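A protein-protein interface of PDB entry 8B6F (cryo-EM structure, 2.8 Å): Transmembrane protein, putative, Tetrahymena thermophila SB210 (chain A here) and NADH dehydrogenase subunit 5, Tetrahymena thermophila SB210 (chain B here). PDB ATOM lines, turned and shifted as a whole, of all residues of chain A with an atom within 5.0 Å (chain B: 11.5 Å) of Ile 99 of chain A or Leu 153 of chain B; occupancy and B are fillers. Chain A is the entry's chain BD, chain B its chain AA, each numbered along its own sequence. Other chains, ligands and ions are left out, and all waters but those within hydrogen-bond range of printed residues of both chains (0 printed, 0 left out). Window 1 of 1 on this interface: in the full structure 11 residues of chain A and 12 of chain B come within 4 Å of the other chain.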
ATOM      1  N   LYS A  95       1.520 -21.876   9.476  1.00  0.00           N
ATOM      2  CA  LYS A  95       2.828 -22.170   8.899  1.00  0.00           C
ATOM      3  C   LYS A  95       3.741 -22.825   9.927  1.00  0.00           C
ATOM      4  O   LYS A  95       4.523 -23.721   9.593  1.00  0.00           O
ATOM      5  CB  LYS A  95       3.460 -20.891   8.354  1.00  0.00           C
ATOM      6  CG  LYS A  95       2.593 -20.167   7.334  1.00  0.00           C
ATOM      7  CD  LYS A  95       3.281 -18.922   6.795  1.00  0.00           C
ATOM      8  CE  LYS A  95       2.349 -18.123   5.900  1.00  0.00           C
ATOM      9  NZ  LYS A  95       1.810 -18.938   4.775  1.00  0.00           N
ATOM     10  N   THR A  96       3.651 -22.395  11.186  1.00  0.00           N
ATOM     11  CA  THR A  96       4.420 -23.040  12.244  1.00  0.00           C
ATOM     12  C   THR A  96       4.026 -24.504  12.381  1.00  0.00           C
ATOM     13  O   THR A  96       4.889 -25.378  12.525  1.00  0.00           O
ATOM     14  CB  THR A  96       4.209 -22.304  13.569  1.00  0.00           C
ATOM     15  OG1 THR A  96       4.771 -20.990  13.484  1.00  0.00           O
ATOM     16  CG2 THR A  96       4.872 -23.054  14.722  1.00  0.00           C
ATOM     17  N   TYR A  97       2.726 -24.790  12.336  1.00  0.00           N
ATOM     18  CA  TYR A  97       2.267 -26.169  12.443  1.00  0.00           C
ATOM     19  C   TYR A  97       2.819 -27.023  11.309  1.00  0.00           C
ATOM     20  O   TYR A  97       3.263 -28.154  11.537  1.00  0.00           O
ATOM     21  CB  TYR A  97       0.739 -26.186  12.448  1.00  0.00           C
ATOM     22  CG  TYR A  97       0.119 -27.560  12.421  1.00  0.00           C
ATOM     23  CD1 TYR A  97      -0.057 -28.291  13.584  1.00  0.00           C
ATOM     24  CD2 TYR A  97      -0.322 -28.112  11.227  1.00  0.00           C
ATOM     25  CE1 TYR A  97      -0.634 -29.542  13.557  1.00  0.00           C
ATOM     26  CE2 TYR A  97      -0.901 -29.359  11.190  1.00  0.00           C
ATOM     27  CZ  TYR A  97      -1.056 -30.070  12.357  1.00  0.00           C
ATOM     28  OH  TYR A  97      -1.633 -31.315  12.317  1.00  0.00           O
ATOM     29  N   TRP A  98       2.800 -26.508  10.081  1.00  0.00           N
ATOM     30  CA  TRP A  98       3.261 -27.300   8.947  1.00  0.00           C
ATOM     31  C   TRP A  98       4.780 -27.409   8.902  1.00  0.00           C
ATOM     32  O   TRP A  98       5.307 -28.421   8.429  1.00  0.00           O
ATOM     33  CB  TRP A  98       2.713 -26.716   7.647  1.00  0.00           C
ATOM     34  CG  TRP A  98       1.264 -27.013   7.502  1.00  0.00           C
ATOM     35  CD1 TRP A  98       0.236 -26.122   7.546  1.00  0.00           C
ATOM     36  CD2 TRP A  98       0.673 -28.305   7.324  1.00  0.00           C
ATOM     37  NE1 TRP A  98      -0.962 -26.779   7.395  1.00  0.00           N
ATOM     38  CE2 TRP A  98      -0.720 -28.119   7.255  1.00  0.00           C
ATOM     39  CE3 TRP A  98       1.190 -29.600   7.209  1.00  0.00           C
ATOM     40  CZ2 TRP A  98      -1.606 -29.180   7.075  1.00  0.00           C
ATOM     41  CZ3 TRP A  98       0.309 -30.652   7.029  1.00  0.00           C
ATOM     42  CH2 TRP A  98      -1.074 -30.435   6.963  1.00  0.00           C
ATOM     43  N   ILE A  99       5.495 -26.391   9.378  1.00  0.00           N
ATOM     44  CA  ILE A  99       6.942 -26.510   9.521  1.00  0.00           C
ATOM     45  C   ILE A  99       7.276 -27.604  10.523  1.00  0.00           C
ATOM     46  O   ILE A  99       8.198 -28.402  10.316  1.00  0.00           O
ATOM     47  CB  ILE A  99       7.554 -25.158   9.928  1.00  0.00           C
ATOM     48  CG1 ILE A  99       7.387 -24.136   8.805  1.00  0.00           C
ATOM     49  CG2 ILE A  99       9.032 -25.313  10.272  1.00  0.00           C
ATOM     50  CD1 ILE A  99       7.473 -22.707   9.278  1.00  0.00           C
ATOM     51  N   THR A 100       6.538 -27.652  11.634  1.00  0.00           N
ATOM     52  CA  THR A 100       6.739 -28.719  12.605  1.00  0.00           C
ATOM     53  C   THR A 100       6.473 -30.081  11.981  1.00  0.00           C
ATOM     54  O   THR A 100       7.224 -31.035  12.210  1.00  0.00           O
ATOM     55  CB  THR A 100       5.831 -28.498  13.816  1.00  0.00           C
ATOM     56  OG1 THR A 100       6.125 -27.229  14.412  1.00  0.00           O
ATOM     57  CG2 THR A 100       6.037 -29.594  14.851  1.00  0.00           C
ATOM     58  N   ASN A 101       5.405 -30.194  11.189  1.00  0.00           N
ATOM     59  CA  ASN A 101       5.108 -31.461  10.533  1.00  0.00           C
ATOM     60  C   ASN A 101       6.233 -31.873   9.595  1.00  0.00           C
ATOM     61  O   ASN A 101       6.639 -33.040   9.577  1.00  0.00           O
ATOM     62  CB  ASN A 101       3.788 -31.360   9.773  1.00  0.00           C
ATOM     63  CG  ASN A 101       2.593 -31.308  10.695  1.00  0.00           C
ATOM     64  OD1 ASN A 101       2.730 -31.069  11.891  1.00  0.00           O
ATOM     65  ND2 ASN A 101       1.409 -31.534  10.141  1.00  0.00           N
ATOM     66  N   ALA A 102       6.746 -30.933   8.801  1.00  0.00           N
ATOM     67  CA  ALA A 102       7.826 -31.266   7.878  1.00  0.00           C
ATOM     68  C   ALA A 102       9.075 -31.703   8.630  1.00  0.00           C
ATOM     69  O   ALA A 102       9.735 -32.674   8.244  1.00  0.00           O
ATOM     70  CB  ALA A 102       8.133 -30.070   6.978  1.00  0.00           C
ATOM     71  N   PHE A 103       9.418 -30.994   9.705  1.00  0.00           N
ATOM     72  CA  PHE A 103      10.570 -31.382  10.510  1.00  0.00           C
ATOM     73  C   PHE A 103      10.377 -32.768  11.109  1.00  0.00           C
ATOM     74  O   PHE A 103      11.310 -33.578  11.135  1.00  0.00           O
ATOM     75  CB  PHE A 103      10.806 -30.342  11.604  1.00  0.00           C
ATOM     76  CG  PHE A 103      11.928 -30.682  12.543  1.00  0.00           C
ATOM     77  CD1 PHE A 103      13.226 -30.290  12.258  1.00  0.00           C
ATOM     78  CD2 PHE A 103      11.683 -31.365  13.724  1.00  0.00           C
ATOM     79  CE1 PHE A 103      14.263 -30.589  13.123  1.00  0.00           C
ATOM     80  CE2 PHE A 103      12.716 -31.667  14.595  1.00  0.00           C
ATOM     81  CZ  PHE A 103      14.008 -31.277  14.293  1.00  0.00           C
ATOM     82  N   ILE A 104       9.171 -33.057  11.603  1.00  0.00           N
ATOM     83  CA  ILE A 104       8.888 -34.379  12.154  1.00  0.00           C
ATOM     84  C   ILE A 104       9.110 -35.452  11.096  1.00  0.00           C
ATOM     85  O   ILE A 104       9.743 -36.481  11.352  1.00  0.00           O
ATOM     86  CB  ILE A 104       7.455 -34.425  12.716  1.00  0.00           C
ATOM     87  CG1 ILE A 104       7.365 -33.603  14.002  1.00  0.00           C
ATOM     88  CG2 ILE A 104       7.012 -35.862  12.974  1.00  0.00           C
ATOM     89  CD1 ILE A 104       5.950 -33.382  14.493  1.00  0.00           C
ATOM     90  N   LEU B  51      23.124 -18.271  -2.702  1.00  0.00           N
ATOM     91  CA  LEU B  51      22.232 -17.805  -1.645  1.00  0.00           C
ATOM     92  C   LEU B  51      22.369 -16.303  -1.431  1.00  0.00           C
ATOM     93  O   LEU B  51      21.369 -15.586  -1.327  1.00  0.00           O
ATOM     94  CB  LEU B  51      22.519 -18.551  -0.343  1.00  0.00           C
ATOM     95  CG  LEU B  51      22.077 -20.009  -0.240  1.00  0.00           C
ATOM     96  CD1 LEU B  51      22.554 -20.565   1.090  1.00  0.00           C
ATOM     97  CD2 LEU B  51      20.570 -20.160  -0.387  1.00  0.00           C
ATOM     98  N   PHE B 144       8.725 -11.866   0.296  1.00  0.00           N
ATOM     99  CA  PHE B 144       9.597 -12.967   0.680  1.00  0.00           C
ATOM    100  C   PHE B 144      11.033 -12.480   0.827  1.00  0.00           C
ATOM    101  O   PHE B 144      11.580 -11.855  -0.086  1.00  0.00           O
ATOM    102  CB  PHE B 144       9.533 -14.098  -0.348  1.00  0.00           C
ATOM    103  CG  PHE B 144      10.446 -15.248  -0.035  1.00  0.00           C
ATOM    104  CD1 PHE B 144      10.045 -16.249   0.833  1.00  0.00           C
ATOM    105  CD2 PHE B 144      11.707 -15.323  -0.604  1.00  0.00           C
ATOM    106  CE1 PHE B 144      10.883 -17.307   1.127  1.00  0.00           C
ATOM    107  CE2 PHE B 144      12.552 -16.378  -0.315  1.00  0.00           C
ATOM    108  CZ  PHE B 144      12.139 -17.372   0.552  1.00  0.00           C
ATOM    109  N   ASN B 145      11.633 -12.769   1.980  1.00  0.00           N
ATOM    110  CA  ASN B 145      13.048 -12.524   2.222  1.00  0.00           C
ATOM    111  C   ASN B 145      13.670 -13.817   2.723  1.00  0.00           C
ATOM    112  O   ASN B 145      13.173 -14.416   3.682  1.00  0.00           O
ATOM    113  CB  ASN B 145      13.247 -11.394   3.237  1.00  0.00           C
ATOM    114  CG  ASN B 145      14.693 -10.960   3.350  1.00  0.00           C
ATOM    115  OD1 ASN B 145      15.538 -11.360   2.548  1.00  0.00           O
ATOM    116  ND2 ASN B 145      14.986 -10.130   4.343  1.00  0.00           N
ATOM    117  N   LEU B 146      14.754 -14.249   2.076  1.00  0.00           N
ATOM    118  CA  LEU B 146      15.324 -15.558   2.383  1.00  0.00           C
ATOM    119  C   LEU B 146      15.833 -15.617   3.817  1.00  0.00           C
ATOM    120  O   LEU B 146      15.580 -16.588   4.537  1.00  0.00           O
ATOM    121  CB  LEU B 146      16.449 -15.886   1.397  1.00  0.00           C
ATOM    122  CG  LEU B 146      17.077 -17.283   1.505  1.00  0.00           C
ATOM    123  CD1 LEU B 146      17.649 -17.703   0.165  1.00  0.00           C
ATOM    124  CD2 LEU B 146      18.172 -17.356   2.568  1.00  0.00           C
ATOM    125  N   PHE B 147      16.556 -14.585   4.254  1.00  0.00           N
ATOM    126  CA  PHE B 147      17.088 -14.596   5.612  1.00  0.00           C
ATOM    127  C   PHE B 147      15.967 -14.601   6.642  1.00  0.00           C
ATOM    128  O   PHE B 147      16.034 -15.326   7.640  1.00  0.00           O
ATOM    129  CB  PHE B 147      18.014 -13.395   5.824  1.00  0.00           C
ATOM    130  CG  PHE B 147      19.288 -13.451   5.015  1.00  0.00           C
ATOM    131  CD1 PHE B 147      19.707 -14.629   4.410  1.00  0.00           C
ATOM    132  CD2 PHE B 147      20.071 -12.317   4.869  1.00  0.00           C
ATOM    133  CE1 PHE B 147      20.878 -14.669   3.673  1.00  0.00           C
ATOM    134  CE2 PHE B 147      21.243 -12.352   4.133  1.00  0.00           C
ATOM    135  CZ  PHE B 147      21.646 -13.529   3.535  1.00  0.00           C
ATOM    136  N   VAL B 148      14.927 -13.797   6.421  1.00  0.00           N
ATOM    137  CA  VAL B 148      13.805 -13.774   7.354  1.00  0.00           C
ATOM    138  C   VAL B 148      13.124 -15.135   7.397  1.00  0.00           C
ATOM    139  O   VAL B 148      12.784 -15.641   8.472  1.00  0.00           O
ATOM    140  CB  VAL B 148      12.815 -12.656   6.973  1.00  0.00           C
ATOM    141  CG1 VAL B 148      11.565 -12.714   7.845  1.00  0.00           C
ATOM    142  CG2 VAL B 148      13.483 -11.297   7.094  1.00  0.00           C
ATOM    143  N   TYR B 149      12.923 -15.755   6.232  1.00  0.00           N
ATOM    144  CA  TYR B 149      12.273 -17.060   6.197  1.00  0.00           C
ATOM    145  C   TYR B 149      13.099 -18.110   6.931  1.00  0.00           C
ATOM    146  O   TYR B 149      12.559 -18.901   7.711  1.00  0.00           O
ATOM    147  CB  TYR B 149      12.027 -17.483   4.750  1.00  0.00           C
ATOM    148  CG  TYR B 149      11.161 -18.715   4.614  1.00  0.00           C
ATOM    149  CD1 TYR B 149       9.799 -18.663   4.885  1.00  0.00           C
ATOM    150  CD2 TYR B 149      11.703 -19.925   4.200  1.00  0.00           C
ATOM    151  CE1 TYR B 149       9.002 -19.784   4.758  1.00  0.00           C
ATOM    152  CE2 TYR B 149      10.913 -21.052   4.069  1.00  0.00           C
ATOM    153  CZ  TYR B 149       9.564 -20.975   4.350  1.00  0.00           C
ATOM    154  OH  TYR B 149       8.773 -22.094   4.221  1.00  0.00           O
ATOM    155  N   ILE B 150      14.414 -18.122   6.706  1.00  0.00           N
ATOM    156  CA  ILE B 150      15.270 -19.095   7.380  1.00  0.00           C
ATOM    157  C   ILE B 150      15.259 -18.853   8.883  1.00  0.00           C
ATOM    158  O   ILE B 150      15.206 -19.797   9.680  1.00  0.00           O
ATOM    159  CB  ILE B 150      16.699 -19.043   6.806  1.00  0.00           C
ATOM    160  CG1 ILE B 150      16.705 -19.472   5.334  1.00  0.00           C
ATOM    161  CG2 ILE B 150      17.649 -19.913   7.634  1.00  0.00           C
ATOM    162  CD1 ILE B 150      16.336 -20.927   5.094  1.00  0.00           C
ATOM    163  N   LYS B 151      15.301 -17.586   9.294  1.00  0.00           N
ATOM    164  CA  LYS B 151      15.264 -17.273  10.718  1.00  0.00           C
ATOM    165  C   LYS B 151      13.949 -17.729  11.336  1.00  0.00           C
ATOM    166  O   LYS B 151      13.933 -18.278  12.442  1.00  0.00           O
ATOM    167  CB  LYS B 151      15.477 -15.774  10.933  1.00  0.00           C
ATOM    168  CG  LYS B 151      15.604 -15.372  12.397  1.00  0.00           C
ATOM    169  CD  LYS B 151      15.962 -13.899  12.555  1.00  0.00           C
ATOM    170  CE  LYS B 151      17.378 -13.609  12.072  1.00  0.00           C
ATOM    171  NZ  LYS B 151      17.790 -12.203  12.348  1.00  0.00           N
ATOM    172  N   THR B 152      12.836 -17.529  10.629  1.00  0.00           N
ATOM    173  CA  THR B 152      11.552 -18.001  11.137  1.00  0.00           C
ATOM    174  C   THR B 152      11.545 -19.519  11.270  1.00  0.00           C
ATOM    175  O   THR B 152      11.053 -20.059  12.268  1.00  0.00           O
ATOM    176  CB  THR B 152      10.416 -17.531  10.229  1.00  0.00           C
ATOM    177  OG1 THR B 152      10.683 -17.914   8.874  1.00  0.00           O
ATOM    178  CG2 THR B 152      10.249 -16.019  10.320  1.00  0.00           C
ATOM    179  N   LEU B 153      12.076 -20.227  10.272  1.00  0.00           N
ATOM    180  CA  LEU B 153      12.134 -21.683  10.358  1.00  0.00           C
ATOM    181  C   LEU B 153      12.963 -22.126  11.558  1.00  0.00           C
ATOM    182  O   LEU B 153      12.597 -23.076  12.259  1.00  0.00           O
ATOM    183  CB  LEU B 153      12.719 -22.264   9.070  1.00  0.00           C
ATOM    184  CG  LEU B 153      11.918 -22.102   7.773  1.00  0.00           C
ATOM    185  CD1 LEU B 153      12.580 -22.879   6.649  1.00  0.00           C
ATOM    186  CD2 LEU B 153      10.470 -22.520   7.934  1.00  0.00           C
ATOM    187  N   LEU B 154      14.090 -21.455  11.805  1.00  0.00           N
ATOM    188  CA  LEU B 154      14.948 -21.819  12.928  1.00  0.00           C
ATOM    189  C   LEU B 154      14.259 -21.548  14.262  1.00  0.00           C
ATOM    190  O   LEU B 154      14.331 -22.372  15.181  1.00  0.00           O
ATOM    191  CB  LEU B 154      16.278 -21.069  12.842  1.00  0.00           C
ATOM    192  CG  LEU B 154      17.430 -21.818  12.158  1.00  0.00           C
ATOM    193  CD1 LEU B 154      17.865 -23.034  12.968  1.00  0.00           C
ATOM    194  CD2 LEU B 154      17.056 -22.227  10.740  1.00  0.00           C
ATOM    195  N   ILE B 155      13.585 -20.402  14.387  1.00  0.00           N
ATOM    196  CA  ILE B 155      12.977 -19.996  15.657  1.00  0.00           C
ATOM    197  C   ILE B 155      11.673 -20.729  15.914  1.00  0.00           C
ATOM    198  O   ILE B 155      11.122 -20.632  17.018  1.00  0.00           O
ATOM    199  CB  ILE B 155      12.762 -18.473  15.726  1.00  0.00           C
ATOM    200  CG1 ILE B 155      11.644 -18.048  14.766  1.00  0.00           C
ATOM    201  CG2 ILE B 155      14.089 -17.747  15.496  1.00  0.00           C
ATOM    202  CD1 ILE B 155      11.518 -16.547  14.568  1.00  0.00           C
ATOM    203  N   THR B 156      11.164 -21.454  14.920  1.00  0.00           N
ATOM    204  CA  THR B 156       9.913 -22.187  15.080  1.00  0.00           C
ATOM    205  C   THR B 156      10.076 -23.241  16.165  1.00  0.00           C
ATOM    206  O   THR B 156       9.162 -23.471  16.966  1.00  0.00           O
ATOM    207  CB  THR B 156       9.490 -22.807  13.743  1.00  0.00           C
ATOM    208  OG1 THR B 156       8.606 -21.908  13.060  1.00  0.00           O
ATOM    209  CG2 THR B 156       8.782 -24.148  13.932  1.00  0.00           C
ATOM    210  N   PHE B 157      11.237 -23.890  16.201  1.00  0.00           N
ATOM    211  CA  PHE B 157      11.548 -24.983  17.112  1.00  0.00           C
ATOM    212  C   PHE B 157      12.207 -24.498  18.397  1.00  0.00           C
ATOM    213  O   PHE B 157      12.560 -25.320  19.249  1.00  0.00           O
ATOM    214  CB  PHE B 157      12.421 -26.015  16.399  1.00  0.00           C
ATOM    215  CG  PHE B 157      11.777 -26.559  15.167  1.00  0.00           C
ATOM    216  CD1 PHE B 157      10.920 -27.641  15.256  1.00  0.00           C
ATOM    217  CD2 PHE B 157      11.958 -25.949  13.937  1.00  0.00           C
ATOM    218  CE1 PHE B 157      10.291 -28.135  14.141  1.00  0.00           C
ATOM    219  CE2 PHE B 157      11.327 -26.439  12.813  1.00  0.00           C
ATOM    220  CZ  PHE B 157      10.493 -27.534  12.916  1.00  0.00           C
ATOM    221  N   ASP B 158      12.389 -23.189  18.541  1.00  0.00           N
ATOM    222  CA  ASP B 158      13.062 -22.616  19.698  1.00  0.00           C
ATOM    223  C   ASP B 158      12.239 -22.932  20.940  1.00  0.00           C
ATOM    224  O   ASP B 158      11.027 -22.704  20.966  1.00  0.00           O
ATOM    225  CB  ASP B 158      13.227 -21.104  19.534  1.00  0.00           C
ATOM    226  CG  ASP B 158      14.134 -20.496  20.587  1.00  0.00           C
ATOM    227  OD1 ASP B 158      14.607 -21.243  21.468  1.00  0.00           O
ATOM    228  OD2 ASP B 158      14.372 -19.272  20.535  1.00  0.00           O
ATOM    229  N   ILE B 159      12.902 -23.442  21.982  1.00  0.00           N
ATOM    230  CA  ILE B 159      12.226 -23.868  23.206  1.00  0.00           C
ATOM    231  C   ILE B 159      12.278 -22.802  24.284  1.00  0.00           C
ATOM    232  O   ILE B 159      11.728 -22.994  25.373  1.00  0.00           O
ATOM    233  CB  ILE B 159      12.809 -25.200  23.718  1.00  0.00           C
ATOM    234  CG1 ILE B 159      14.305 -25.072  24.010  1.00  0.00           C
ATOM    235  CG2 ILE B 159      12.562 -26.302  22.707  1.00  0.00           C
ATOM    236  CD1 ILE B 159      14.755 -25.924  25.168  1.00  0.00           C
ATOM    237  N   GLN B 161      10.882 -19.994  24.066  1.00  0.00           N
ATOM    238  CA  GLN B 161       9.558 -19.381  24.027  1.00  0.00           C
ATOM    239  C   GLN B 161       8.586 -20.018  25.017  1.00  0.00           C
ATOM    240  O   GLN B 161       7.744 -19.312  25.585  1.00  0.00           O
ATOM    241  CB  GLN B 161       8.998 -19.509  22.609  1.00  0.00           C
ATOM    242  CG  GLN B 161       9.884 -18.917  21.523  1.00  0.00           C
ATOM    243  CD  GLN B 161      10.658 -17.709  21.996  1.00  0.00           C
ATOM    244  OE1 GLN B 161      11.861 -17.782  22.248  1.00  0.00           O
ATOM    245  NE2 GLN B 161       9.968 -16.583  22.124  1.00  0.00           N
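Among the printed residues, pairs that only touch across the chains: Thr 96 of chain A with Thr 156 of chain B (3.97 Å), Ile 99 of chain A with Leu 153 of chain B (3.3 Å), Ile 99 of chain A with Thr 156 of chain B (3.8 Å), Ile 99 of chain A with Phe 157 of chain B (3.6 Å), Thr 100 of chain A with Phe 157 of chain B (3.9 Å) and Phe 103 of chain A with Phe 157 of chain B (3.1 Å).
The backbone carbonyl oxygen of Thr 152 of chain B lies within hydrogen-bond range of the side-chain hydroxyl of Thr 156 of chain B.
O of Thr 96 of chain A sits at hydrogen-bond distance from OG1 of Thr 100 of chain A (2.9 Å).
Of the 10 printed residues of chain A, 4 touch a printed residue of chain B.
Among the printed residues, 6 pairs touch across the chains.
Ile 99 of chain A touches three residues of chain B.
Of chain A, only Ile 99 comes within 4 Å of Leu 153 of chain B.
Of chain B, only Thr 156 (3.97 Å) comes within 4 Å of Thr 96 of chain A.
Of the printed residues of chain A, Thr 156 of chain B touches Thr 96 and Ile 99.
Of the printed residues of chain A, Phe 157 of chain B touches Ile 99, Thr 100 and Phe 103.
Of the printed residues of chain B, Phe 103 of chain A touches Phe 157.
Asn 145 of chain B touches none of the printed residues of chain A.
Lys 151 of chain B touches none of the printed residues of chain A.
The nearest residue of chain B that does not touch Ile 99 of chain A is Tyr 149 of chain B (5.2 Å).
The nearest printed residue of chain A that does not touch Leu 153 of chain B is Lys 95 of chain A (6.3 Å).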
